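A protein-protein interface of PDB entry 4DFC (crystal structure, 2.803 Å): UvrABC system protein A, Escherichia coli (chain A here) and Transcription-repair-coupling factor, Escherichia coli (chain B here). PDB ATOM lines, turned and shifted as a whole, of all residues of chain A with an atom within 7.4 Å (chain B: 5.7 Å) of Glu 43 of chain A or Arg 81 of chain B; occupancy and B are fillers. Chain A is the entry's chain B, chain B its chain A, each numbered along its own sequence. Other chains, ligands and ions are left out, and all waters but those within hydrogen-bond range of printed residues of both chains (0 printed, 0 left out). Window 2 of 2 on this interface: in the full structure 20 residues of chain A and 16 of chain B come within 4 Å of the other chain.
The side-chain carboxylate (OE2) of Glu 43 of chain A is in salt-bridge range of the guanidinium group (NH1) of Arg 81 of chain B, 3.7 Å away. The guanidinium group of Arg 61 of chain B sits close to the backbone carbonyl oxygen of Gly 49 of chain A (3.4 Å). The backbone carbonyl oxygen (O) of Ala 46 of chain A lies close to the backbone carbonyl oxygen (O) of Gln 80 of chain B.
The side-chain hydroxyl (OG) of Ser 47 of chain A sits at hydrogen-bond distance from the backbone carbonyl oxygen (O) of Glu 43 of chain A, 3.1 Å away. OG of Ser 79 of chain B sits close to N of Arg 81 of chain B, at 3.4 Å. The backbone NH (N) of Asp 76 of chain B is in hydrogen-bond range of the backbone carbonyl oxygen (O) of Arg 81 of chain B (3.2 Å). NH2 of Arg 61 of chain B is in hydrogen-bond range of O of Gln 80 of chain B. O of Ile 51 of chain A sits at hydrogen-bond distance from N of Leu 62 of chain A, 2.6 Å away. The side-chain carboxylate of Asp 76 of chain B sits at hydrogen-bond distance from the backbone NH of Ser 79 of chain B (2.9 Å).
Among the printed residues, merely in contact across the chains: Ile 51 of chain A with Thr 82 of chain B (3.3 Å), Ser 47 of chain A with Gln 80 of chain B (3.3 Å), Ala 46 of chain A with Arg 81 of chain B (3.4 Å), Ile 51 of chain A with Arg 61 of chain B (3.7 Å), Ser 47 of chain A with Ser 79 of chain B (3.7 Å), Leu 62 of chain A with Arg 81 of chain B (3.8 Å) and Gly 49 of chain A with Gln 80 of chain B (3.8 Å).
Glu 43 of chain A touches just one residue of chain B: Arg 81 (3.7 Å). Asp 76 of chain B touches none of the printed residues of chain A. Printed residues of chain A within 4 Å of Ser 79 of chain B: Ser 47. Arg 81 of chain B touches just these residues of chain A: Glu 43, Ala 46 and Leu 62. Of the printed residues of chain A, Thr 82 of chain B touches Ile 51 (3.3 Å). Leu 83 of chain B touches none of the printed residues of chain A. The nearest residue of chain A that does not touch Arg 81 of chain B is Ser 47 of chain A (4.1 Å).
Of the 9 printed residues of chain B, 5 touch a printed residue of chain A. Printed residues of chain A that touch a printed residue of chain B: Glu 43, Ala 46, Ser 47, Gly 49, Ile 51 and Leu 62. Hydrophobic or aromatic side chains of chain A that line the printed part of chain B: Ala 46 and Ile 51. Among the printed residues, Asp or Glu carboxylates within 4 Å of a Lys or Arg side-chain nitrogen of the other chain: Glu 43 of chain A with Arg 81 of chain B.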
ATOM      1  N   HIS A  38      -3.365 -11.925  19.640  1.00  0.00           N
ATOM      2  CA  HIS A  38      -4.288 -10.809  19.460  1.00  0.00           C
ATOM      3  C   HIS A  38      -5.706 -11.236  19.084  1.00  0.00           C
ATOM      4  O   HIS A  38      -6.429 -10.494  18.417  1.00  0.00           O
ATOM      5  CB  HIS A  38      -3.718  -9.825  18.426  1.00  0.00           C
ATOM      6  CG  HIS A  38      -2.337  -9.355  18.754  1.00  0.00           C
ATOM      7  ND1 HIS A  38      -2.096  -8.297  19.605  1.00  0.00           N
ATOM      8  CD2 HIS A  38      -1.121  -9.823  18.378  1.00  0.00           C
ATOM      9  CE1 HIS A  38      -0.790  -8.129  19.733  1.00  0.00           C
ATOM     10  NE2 HIS A  38      -0.175  -9.040  18.997  1.00  0.00           N
ATOM     11  N   THR A  39      -6.114 -12.415  19.540  1.00  0.00           N
ATOM     12  CA  THR A  39      -7.461 -12.919  19.269  1.00  0.00           C
ATOM     13  C   THR A  39      -8.531 -11.984  19.845  1.00  0.00           C
ATOM     14  O   THR A  39      -9.643 -11.900  19.324  1.00  0.00           O
ATOM     15  CB  THR A  39      -7.654 -14.359  19.823  1.00  0.00           C
ATOM     16  OG1 THR A  39      -7.179 -14.441  21.180  1.00  0.00           O
ATOM     17  CG2 THR A  39      -6.883 -15.356  18.995  1.00  0.00           C
ATOM     18  N   LYS A  40      -8.185 -11.274  20.916  1.00  0.00           N
ATOM     19  CA  LYS A  40      -9.159 -10.453  21.635  1.00  0.00           C
ATOM     20  C   LYS A  40      -9.454  -9.112  20.957  1.00  0.00           C
ATOM     21  O   LYS A  40     -10.621  -8.731  20.857  1.00  0.00           O
ATOM     22  CB  LYS A  40      -8.730 -10.235  23.093  1.00  0.00           C
ATOM     23  CG  LYS A  40      -9.834  -9.737  24.028  1.00  0.00           C
ATOM     24  CD  LYS A  40      -9.231  -9.102  25.278  1.00  0.00           C
ATOM     25  CE  LYS A  40     -10.275  -8.506  26.211  1.00  0.00           C
ATOM     26  NZ  LYS A  40      -9.541  -7.755  27.288  1.00  0.00           N
ATOM     27  N   THR A  41      -8.414  -8.390  20.520  1.00  0.00           N
ATOM     28  CA  THR A  41      -8.631  -7.141  19.778  1.00  0.00           C
ATOM     29  C   THR A  41      -9.230  -7.441  18.400  1.00  0.00           C
ATOM     30  O   THR A  41     -10.163  -6.756  17.961  1.00  0.00           O
ATOM     31  CB  THR A  41      -7.356  -6.255  19.619  1.00  0.00           C
ATOM     32  OG1 THR A  41      -6.261  -7.064  19.219  1.00  0.00           O
ATOM     33  CG2 THR A  41      -6.989  -5.510  20.924  1.00  0.00           C
ATOM     34  N   LEU A  42      -8.711  -8.478  17.739  1.00  0.00           N
ATOM     35  CA  LEU A  42      -9.234  -8.895  16.437  1.00  0.00           C
ATOM     36  C   LEU A  42     -10.704  -9.246  16.533  1.00  0.00           C
ATOM     37  O   LEU A  42     -11.448  -9.151  15.552  1.00  0.00           O
ATOM     38  CB  LEU A  42      -8.474 -10.105  15.896  1.00  0.00           C
ATOM     39  CG  LEU A  42      -7.205  -9.871  15.081  1.00  0.00           C
ATOM     40  CD1 LEU A  42      -6.572 -11.195  14.687  1.00  0.00           C
ATOM     41  CD2 LEU A  42      -7.513  -9.042  13.856  1.00  0.00           C
ATOM     42  N   GLU A  43     -11.105  -9.712  17.707  1.00  0.00           N
ATOM     43  CA  GLU A  43     -12.492 -10.066  17.948  1.00  0.00           C
ATOM     44  C   GLU A  43     -13.270  -8.790  18.286  1.00  0.00           C
ATOM     45  O   GLU A  43     -14.422  -8.600  17.877  1.00  0.00           O
ATOM     46  CB  GLU A  43     -12.576 -11.110  19.073  1.00  0.00           C
ATOM     47  CG  GLU A  43     -13.906 -11.833  19.169  1.00  0.00           C
ATOM     48  CD  GLU A  43     -14.950 -11.015  19.908  1.00  0.00           C
ATOM     49  OE1 GLU A  43     -14.562 -10.078  20.656  1.00  0.00           O
ATOM     50  OE2 GLU A  43     -16.155 -11.311  19.736  1.00  0.00           O
ATOM     51  N   ASN A  44     -12.617  -7.917  19.042  1.00  0.00           N
ATOM     52  CA  ASN A  44     -13.225  -6.681  19.479  1.00  0.00           C
ATOM     53  C   ASN A  44     -13.444  -5.731  18.294  1.00  0.00           C
ATOM     54  O   ASN A  44     -14.504  -5.098  18.203  1.00  0.00           O
ATOM     55  CB  ASN A  44     -12.397  -6.050  20.602  1.00  0.00           C
ATOM     56  CG  ASN A  44     -12.565  -4.536  20.691  1.00  0.00           C
ATOM     57  OD1 ASN A  44     -11.757  -3.778  20.139  1.00  0.00           O
ATOM     58  ND2 ASN A  44     -13.602  -4.087  21.400  1.00  0.00           N
ATOM     59  N   LEU A  45     -12.469  -5.661  17.378  1.00  0.00           N
ATOM     60  CA  LEU A  45     -12.615  -4.850  16.158  1.00  0.00           C
ATOM     61  C   LEU A  45     -13.790  -5.332  15.316  1.00  0.00           C
ATOM     62  O   LEU A  45     -14.528  -4.524  14.746  1.00  0.00           O
ATOM     63  CB  LEU A  45     -11.334  -4.836  15.303  1.00  0.00           C
ATOM     64  CG  LEU A  45     -10.101  -4.257  15.992  1.00  0.00           C
ATOM     65  CD1 LEU A  45      -8.866  -4.372  15.126  1.00  0.00           C
ATOM     66  CD2 LEU A  45     -10.353  -2.826  16.413  1.00  0.00           C
ATOM     67  N   ALA A  46     -13.971  -6.646  15.238  1.00  0.00           N
ATOM     68  CA  ALA A  46     -15.063  -7.168  14.435  1.00  0.00           C
ATOM     69  C   ALA A  46     -16.400  -6.784  15.042  1.00  0.00           C
ATOM     70  O   ALA A  46     -17.382  -6.635  14.329  1.00  0.00           O
ATOM     71  CB  ALA A  46     -14.956  -8.669  14.275  1.00  0.00           C
ATOM     72  N   SER A  47     -16.429  -6.619  16.361  1.00  0.00           N
ATOM     73  CA  SER A  47     -17.678  -6.369  17.073  1.00  0.00           C
ATOM     74  C   SER A  47     -18.059  -4.901  17.024  1.00  0.00           C
ATOM     75  O   SER A  47     -19.218  -4.545  17.224  1.00  0.00           O
ATOM     76  CB  SER A  47     -17.578  -6.858  18.522  1.00  0.00           C
ATOM     77  OG  SER A  47     -17.395  -8.273  18.573  1.00  0.00           O
ATOM     78  N   GLN A  48     -17.074  -4.055  16.745  1.00  0.00           N
ATOM     79  CA  GLN A  48     -17.292  -2.621  16.616  1.00  0.00           C
ATOM     80  C   GLN A  48     -17.946  -2.323  15.269  1.00  0.00           C
ATOM     81  O   GLN A  48     -18.531  -1.249  15.066  1.00  0.00           O
ATOM     82  CB  GLN A  48     -15.968  -1.863  16.758  1.00  0.00           C
ATOM     83  CG  GLN A  48     -15.271  -2.071  18.107  1.00  0.00           C
ATOM     84  CD  GLN A  48     -14.506  -0.850  18.551  1.00  0.00           C
ATOM     85  OE1 GLN A  48     -14.977   0.275  18.376  1.00  0.00           O
ATOM     86  NE2 GLN A  48     -13.323  -1.055  19.129  1.00  0.00           N
ATOM     87  N   GLY A  49     -17.875  -3.299  14.368  1.00  0.00           N
ATOM     88  CA  GLY A  49     -18.496  -3.189  13.059  1.00  0.00           C
ATOM     89  C   GLY A  49     -17.556  -3.062  11.868  1.00  0.00           C
ATOM     90  O   GLY A  49     -18.009  -3.110  10.733  1.00  0.00           O
ATOM     91  N   TYR A  50     -16.256  -2.917  12.112  1.00  0.00           N
ATOM     92  CA  TYR A  50     -15.288  -2.827  11.024  1.00  0.00           C
ATOM     93  C   TYR A  50     -15.119  -4.144  10.255  1.00  0.00           C
ATOM     94  O   TYR A  50     -15.419  -5.215  10.778  1.00  0.00           O
ATOM     95  CB  TYR A  50     -13.962  -2.239  11.521  1.00  0.00           C
ATOM     96  CG  TYR A  50     -14.173  -0.892  12.185  1.00  0.00           C
ATOM     97  CD1 TYR A  50     -14.284   0.275  11.437  1.00  0.00           C
ATOM     98  CD2 TYR A  50     -14.314  -0.795  13.552  1.00  0.00           C
ATOM     99  CE1 TYR A  50     -14.507   1.513  12.046  1.00  0.00           C
ATOM    100  CE2 TYR A  50     -14.531   0.422  14.168  1.00  0.00           C
ATOM    101  CZ  TYR A  50     -14.630   1.572  13.416  1.00  0.00           C
ATOM    102  OH  TYR A  50     -14.853   2.764  14.067  1.00  0.00           O
ATOM    103  N   ILE A  51     -14.678  -4.038   9.000  1.00  0.00           N
ATOM    104  CA  ILE A  51     -14.601  -5.158   8.050  1.00  0.00           C
ATOM    105  C   ILE A  51     -13.183  -5.477   7.577  1.00  0.00           C
ATOM    106  O   ILE A  51     -12.821  -6.633   7.417  1.00  0.00           O
ATOM    107  CB  ILE A  51     -15.589  -5.060   6.869  1.00  0.00           C
ATOM    108  CG1 ILE A  51     -15.301  -3.838   5.991  1.00  0.00           C
ATOM    109  CG2 ILE A  51     -17.008  -5.009   7.385  1.00  0.00           C
ATOM    110  CD1 ILE A  51     -16.088  -3.822   4.682  1.00  0.00           C
ATOM    111  N   LEU A  62     -11.980  -8.839   8.544  1.00  0.00           N
ATOM    112  CA  LEU A  62     -12.032  -8.975  10.003  1.00  0.00           C
ATOM    113  C   LEU A  62     -13.050 -10.021  10.462  1.00  0.00           C
ATOM    114  O   LEU A  62     -13.128 -10.348  11.657  1.00  0.00           O
ATOM    115  CB  LEU A  62     -12.330  -7.632  10.685  1.00  0.00           C
ATOM    116  CG  LEU A  62     -11.148  -6.665  10.874  1.00  0.00           C
ATOM    117  CD1 LEU A  62     -11.602  -5.318  11.409  1.00  0.00           C
ATOM    118  CD2 LEU A  62     -10.061  -7.231  11.770  1.00  0.00           C
ATOM    119  N   SER A  63     -13.836 -10.521   9.512  1.00  0.00           N
ATOM    120  CA  SER A  63     -14.837 -11.544   9.778  1.00  0.00           C
ATOM    121  C   SER A  63     -14.183 -12.921   9.799  1.00  0.00           C
ATOM    122  O   SER A  63     -14.674 -13.855  10.441  1.00  0.00           O
ATOM    123  CB  SER A  63     -15.938 -11.498   8.715  1.00  0.00           C
ATOM    124  OG  SER A  63     -15.637 -12.362   7.637  1.00  0.00           O
ATOM    125  N   ASP A  64     -13.079 -13.022   9.064  1.00  0.00           N
ATOM    126  CA  ASP A  64     -12.283 -14.237   8.936  1.00  0.00           C
ATOM    127  C   ASP A  64     -10.803 -13.847   8.877  1.00  0.00           C
ATOM    128  O   ASP A  64     -10.178 -13.941   7.824  1.00  0.00           O
ATOM    129  CB  ASP A  64     -12.684 -14.985   7.656  1.00  0.00           C
ATOM    130  CG  ASP A  64     -11.794 -16.189   7.368  1.00  0.00           C
ATOM    131  OD1 ASP A  64     -11.475 -16.931   8.329  1.00  0.00           O
ATOM    132  OD2 ASP A  64     -11.422 -16.387   6.180  1.00  0.00           O
ATOM    133  N   PRO A  65     -10.243 -13.384  10.004  1.00  0.00           N
ATOM    134  CA  PRO A  65      -8.847 -12.938  10.067  1.00  0.00           C
ATOM    135  C   PRO A  65      -7.878 -14.074   9.825  1.00  0.00           C
ATOM    136  O   PRO A  65      -8.251 -15.242   9.943  1.00  0.00           O
ATOM    137  CB  PRO A  65      -8.685 -12.485  11.518  1.00  0.00           C
ATOM    138  CG  PRO A  65     -10.074 -12.239  12.023  1.00  0.00           C
ATOM    139  CD  PRO A  65     -10.943 -13.208  11.287  1.00  0.00           C
ATOM    140  N   ARG B  61     -24.927  -3.450   5.285  1.00  0.00           N
ATOM    141  CA  ARG B  61     -23.695  -2.708   5.537  1.00  0.00           C
ATOM    142  C   ARG B  61     -22.979  -2.390   4.219  1.00  0.00           C
ATOM    143  O   ARG B  61     -22.456  -3.289   3.556  1.00  0.00           O
ATOM    144  CB  ARG B  61     -22.762  -3.505   6.468  1.00  0.00           C
ATOM    145  CG  ARG B  61     -21.307  -3.068   6.382  1.00  0.00           C
ATOM    146  CD  ARG B  61     -20.420  -3.691   7.425  1.00  0.00           C
ATOM    147  NE  ARG B  61     -20.851  -3.349   8.774  1.00  0.00           N
ATOM    148  CZ  ARG B  61     -20.912  -4.224   9.774  1.00  0.00           C
ATOM    149  NH1 ARG B  61     -20.566  -5.488   9.575  1.00  0.00           N
ATOM    150  NH2 ARG B  61     -21.312  -3.838  10.977  1.00  0.00           N
ATOM    151  N   VAL B  74     -24.804  -8.209   4.129  1.00  0.00           N
ATOM    152  CA  VAL B  74     -25.716  -8.390   5.250  1.00  0.00           C
ATOM    153  C   VAL B  74     -24.889  -8.557   6.519  1.00  0.00           C
ATOM    154  O   VAL B  74     -23.760  -9.058   6.488  1.00  0.00           O
ATOM    155  CB  VAL B  74     -26.599  -9.630   5.099  1.00  0.00           C
ATOM    156  CG1 VAL B  74     -27.650  -9.635   6.188  1.00  0.00           C
ATOM    157  CG2 VAL B  74     -27.250  -9.673   3.722  1.00  0.00           C
ATOM    158  N   PHE B  75     -25.442  -8.126   7.639  1.00  0.00           N
ATOM    159  CA  PHE B  75     -24.738  -8.256   8.898  1.00  0.00           C
ATOM    160  C   PHE B  75     -25.746  -8.541   9.986  1.00  0.00           C
ATOM    161  O   PHE B  75     -26.915  -8.166   9.869  1.00  0.00           O
ATOM    162  CB  PHE B  75     -23.906  -7.009   9.212  1.00  0.00           C
ATOM    163  CG  PHE B  75     -24.715  -5.834   9.690  1.00  0.00           C
ATOM    164  CD1 PHE B  75     -24.815  -5.552  11.037  1.00  0.00           C
ATOM    165  CD2 PHE B  75     -25.366  -5.006   8.793  1.00  0.00           C
ATOM    166  CE1 PHE B  75     -25.556  -4.475  11.480  1.00  0.00           C
ATOM    167  CE2 PHE B  75     -26.108  -3.926   9.235  1.00  0.00           C
ATOM    168  CZ  PHE B  75     -26.200  -3.660  10.579  1.00  0.00           C
ATOM    169  N   ASP B  76     -25.282  -9.236  11.020  1.00  0.00           N
ATOM    170  CA  ASP B  76     -26.102  -9.624  12.157  1.00  0.00           C
ATOM    171  C   ASP B  76     -26.061  -8.523  13.224  1.00  0.00           C
ATOM    172  O   ASP B  76     -24.985  -8.059  13.611  1.00  0.00           O
ATOM    173  CB  ASP B  76     -25.572 -10.951  12.717  1.00  0.00           C
ATOM    174  CG  ASP B  76     -26.269 -11.365  13.982  1.00  0.00           C
ATOM    175  OD1 ASP B  76     -25.817 -10.924  15.059  1.00  0.00           O
ATOM    176  OD2 ASP B  76     -27.260 -12.126  13.902  1.00  0.00           O
ATOM    177  N   SER B  79     -23.908  -9.723  16.821  1.00  0.00           N
ATOM    178  CA  SER B  79     -22.447  -9.797  16.672  1.00  0.00           C
ATOM    179  C   SER B  79     -21.872  -8.588  15.961  1.00  0.00           C
ATOM    180  O   SER B  79     -20.681  -8.298  16.102  1.00  0.00           O
ATOM    181  CB  SER B  79     -22.013 -11.064  15.919  1.00  0.00           C
ATOM    182  OG  SER B  79     -22.552 -11.134  14.612  1.00  0.00           O
ATOM    183  N   GLN B  80     -22.717  -7.900  15.190  1.00  0.00           N
ATOM    184  CA  GLN B  80     -22.286  -6.768  14.368  1.00  0.00           C
ATOM    185  C   GLN B  80     -21.311  -7.203  13.276  1.00  0.00           C
ATOM    186  O   GLN B  80     -20.509  -6.401  12.806  1.00  0.00           O
ATOM    187  CB  GLN B  80     -21.641  -5.689  15.237  1.00  0.00           C
ATOM    188  CG  GLN B  80     -22.620  -4.943  16.106  1.00  0.00           C
ATOM    189  CD  GLN B  80     -23.274  -3.790  15.371  1.00  0.00           C
ATOM    190  OE1 GLN B  80     -22.592  -2.874  14.900  1.00  0.00           O
ATOM    191  NE2 GLN B  80     -24.604  -3.829  15.265  1.00  0.00           N
ATOM    192  N   ARG B  81     -21.396  -8.465  12.862  1.00  0.00           N
ATOM    193  CA  ARG B  81     -20.433  -9.028  11.917  1.00  0.00           C
ATOM    194  C   ARG B  81     -20.994  -9.269  10.509  1.00  0.00           C
ATOM    195  O   ARG B  81     -22.157  -9.635  10.327  1.00  0.00           O
ATOM    196  CB  ARG B  81     -19.816 -10.311  12.489  1.00  0.00           C
ATOM    197  CG  ARG B  81     -19.042 -10.103  13.783  1.00  0.00           C
ATOM    198  CD  ARG B  81     -18.636 -11.425  14.382  1.00  0.00           C
ATOM    199  NE  ARG B  81     -17.299 -11.847  13.974  1.00  0.00           N
ATOM    200  CZ  ARG B  81     -16.237 -11.820  14.776  1.00  0.00           C
ATOM    201  NH1 ARG B  81     -16.363 -11.382  16.028  1.00  0.00           N
ATOM    202  NH2 ARG B  81     -15.051 -12.231  14.332  1.00  0.00           N
ATOM    203  N   THR B  82     -20.138  -9.075   9.516  1.00  0.00           N
ATOM    204  CA  THR B  82     -20.546  -9.111   8.121  1.00  0.00           C
ATOM    205  C   THR B  82     -20.815 -10.544   7.671  1.00  0.00           C
ATOM    206  O   THR B  82     -19.938 -11.403   7.742  1.00  0.00           O
ATOM    207  CB  THR B  82     -19.426  -8.515   7.248  1.00  0.00           C
ATOM    208  OG1 THR B  82     -18.823  -9.547   6.455  1.00  0.00           O
ATOM    209  CG2 THR B  82     -18.345  -7.900   8.139  1.00  0.00           C
ATOM    210  N   LEU B  83     -22.031 -10.795   7.208  1.00  0.00           N
ATOM    211  CA  LEU B  83     -22.384 -12.066   6.566  1.00  0.00           C
ATOM    212  C   LEU B  83     -22.160 -11.980   5.052  1.00  0.00           C
ATOM    213  O   LEU B  83     -21.411 -11.125   4.576  1.00  0.00           O
ATOM    214  CB  LEU B  83     -23.819 -12.471   6.883  1.00  0.00           C
ATOM    215  CG  LEU B  83     -24.182 -12.336   8.364  1.00  0.00           C
ATOM    216  CD1 LEU B  83     -25.657 -12.682   8.620  1.00  0.00           C
ATOM    217  CD2 LEU B  83     -23.253 -13.195   9.204  1.00  0.00           C
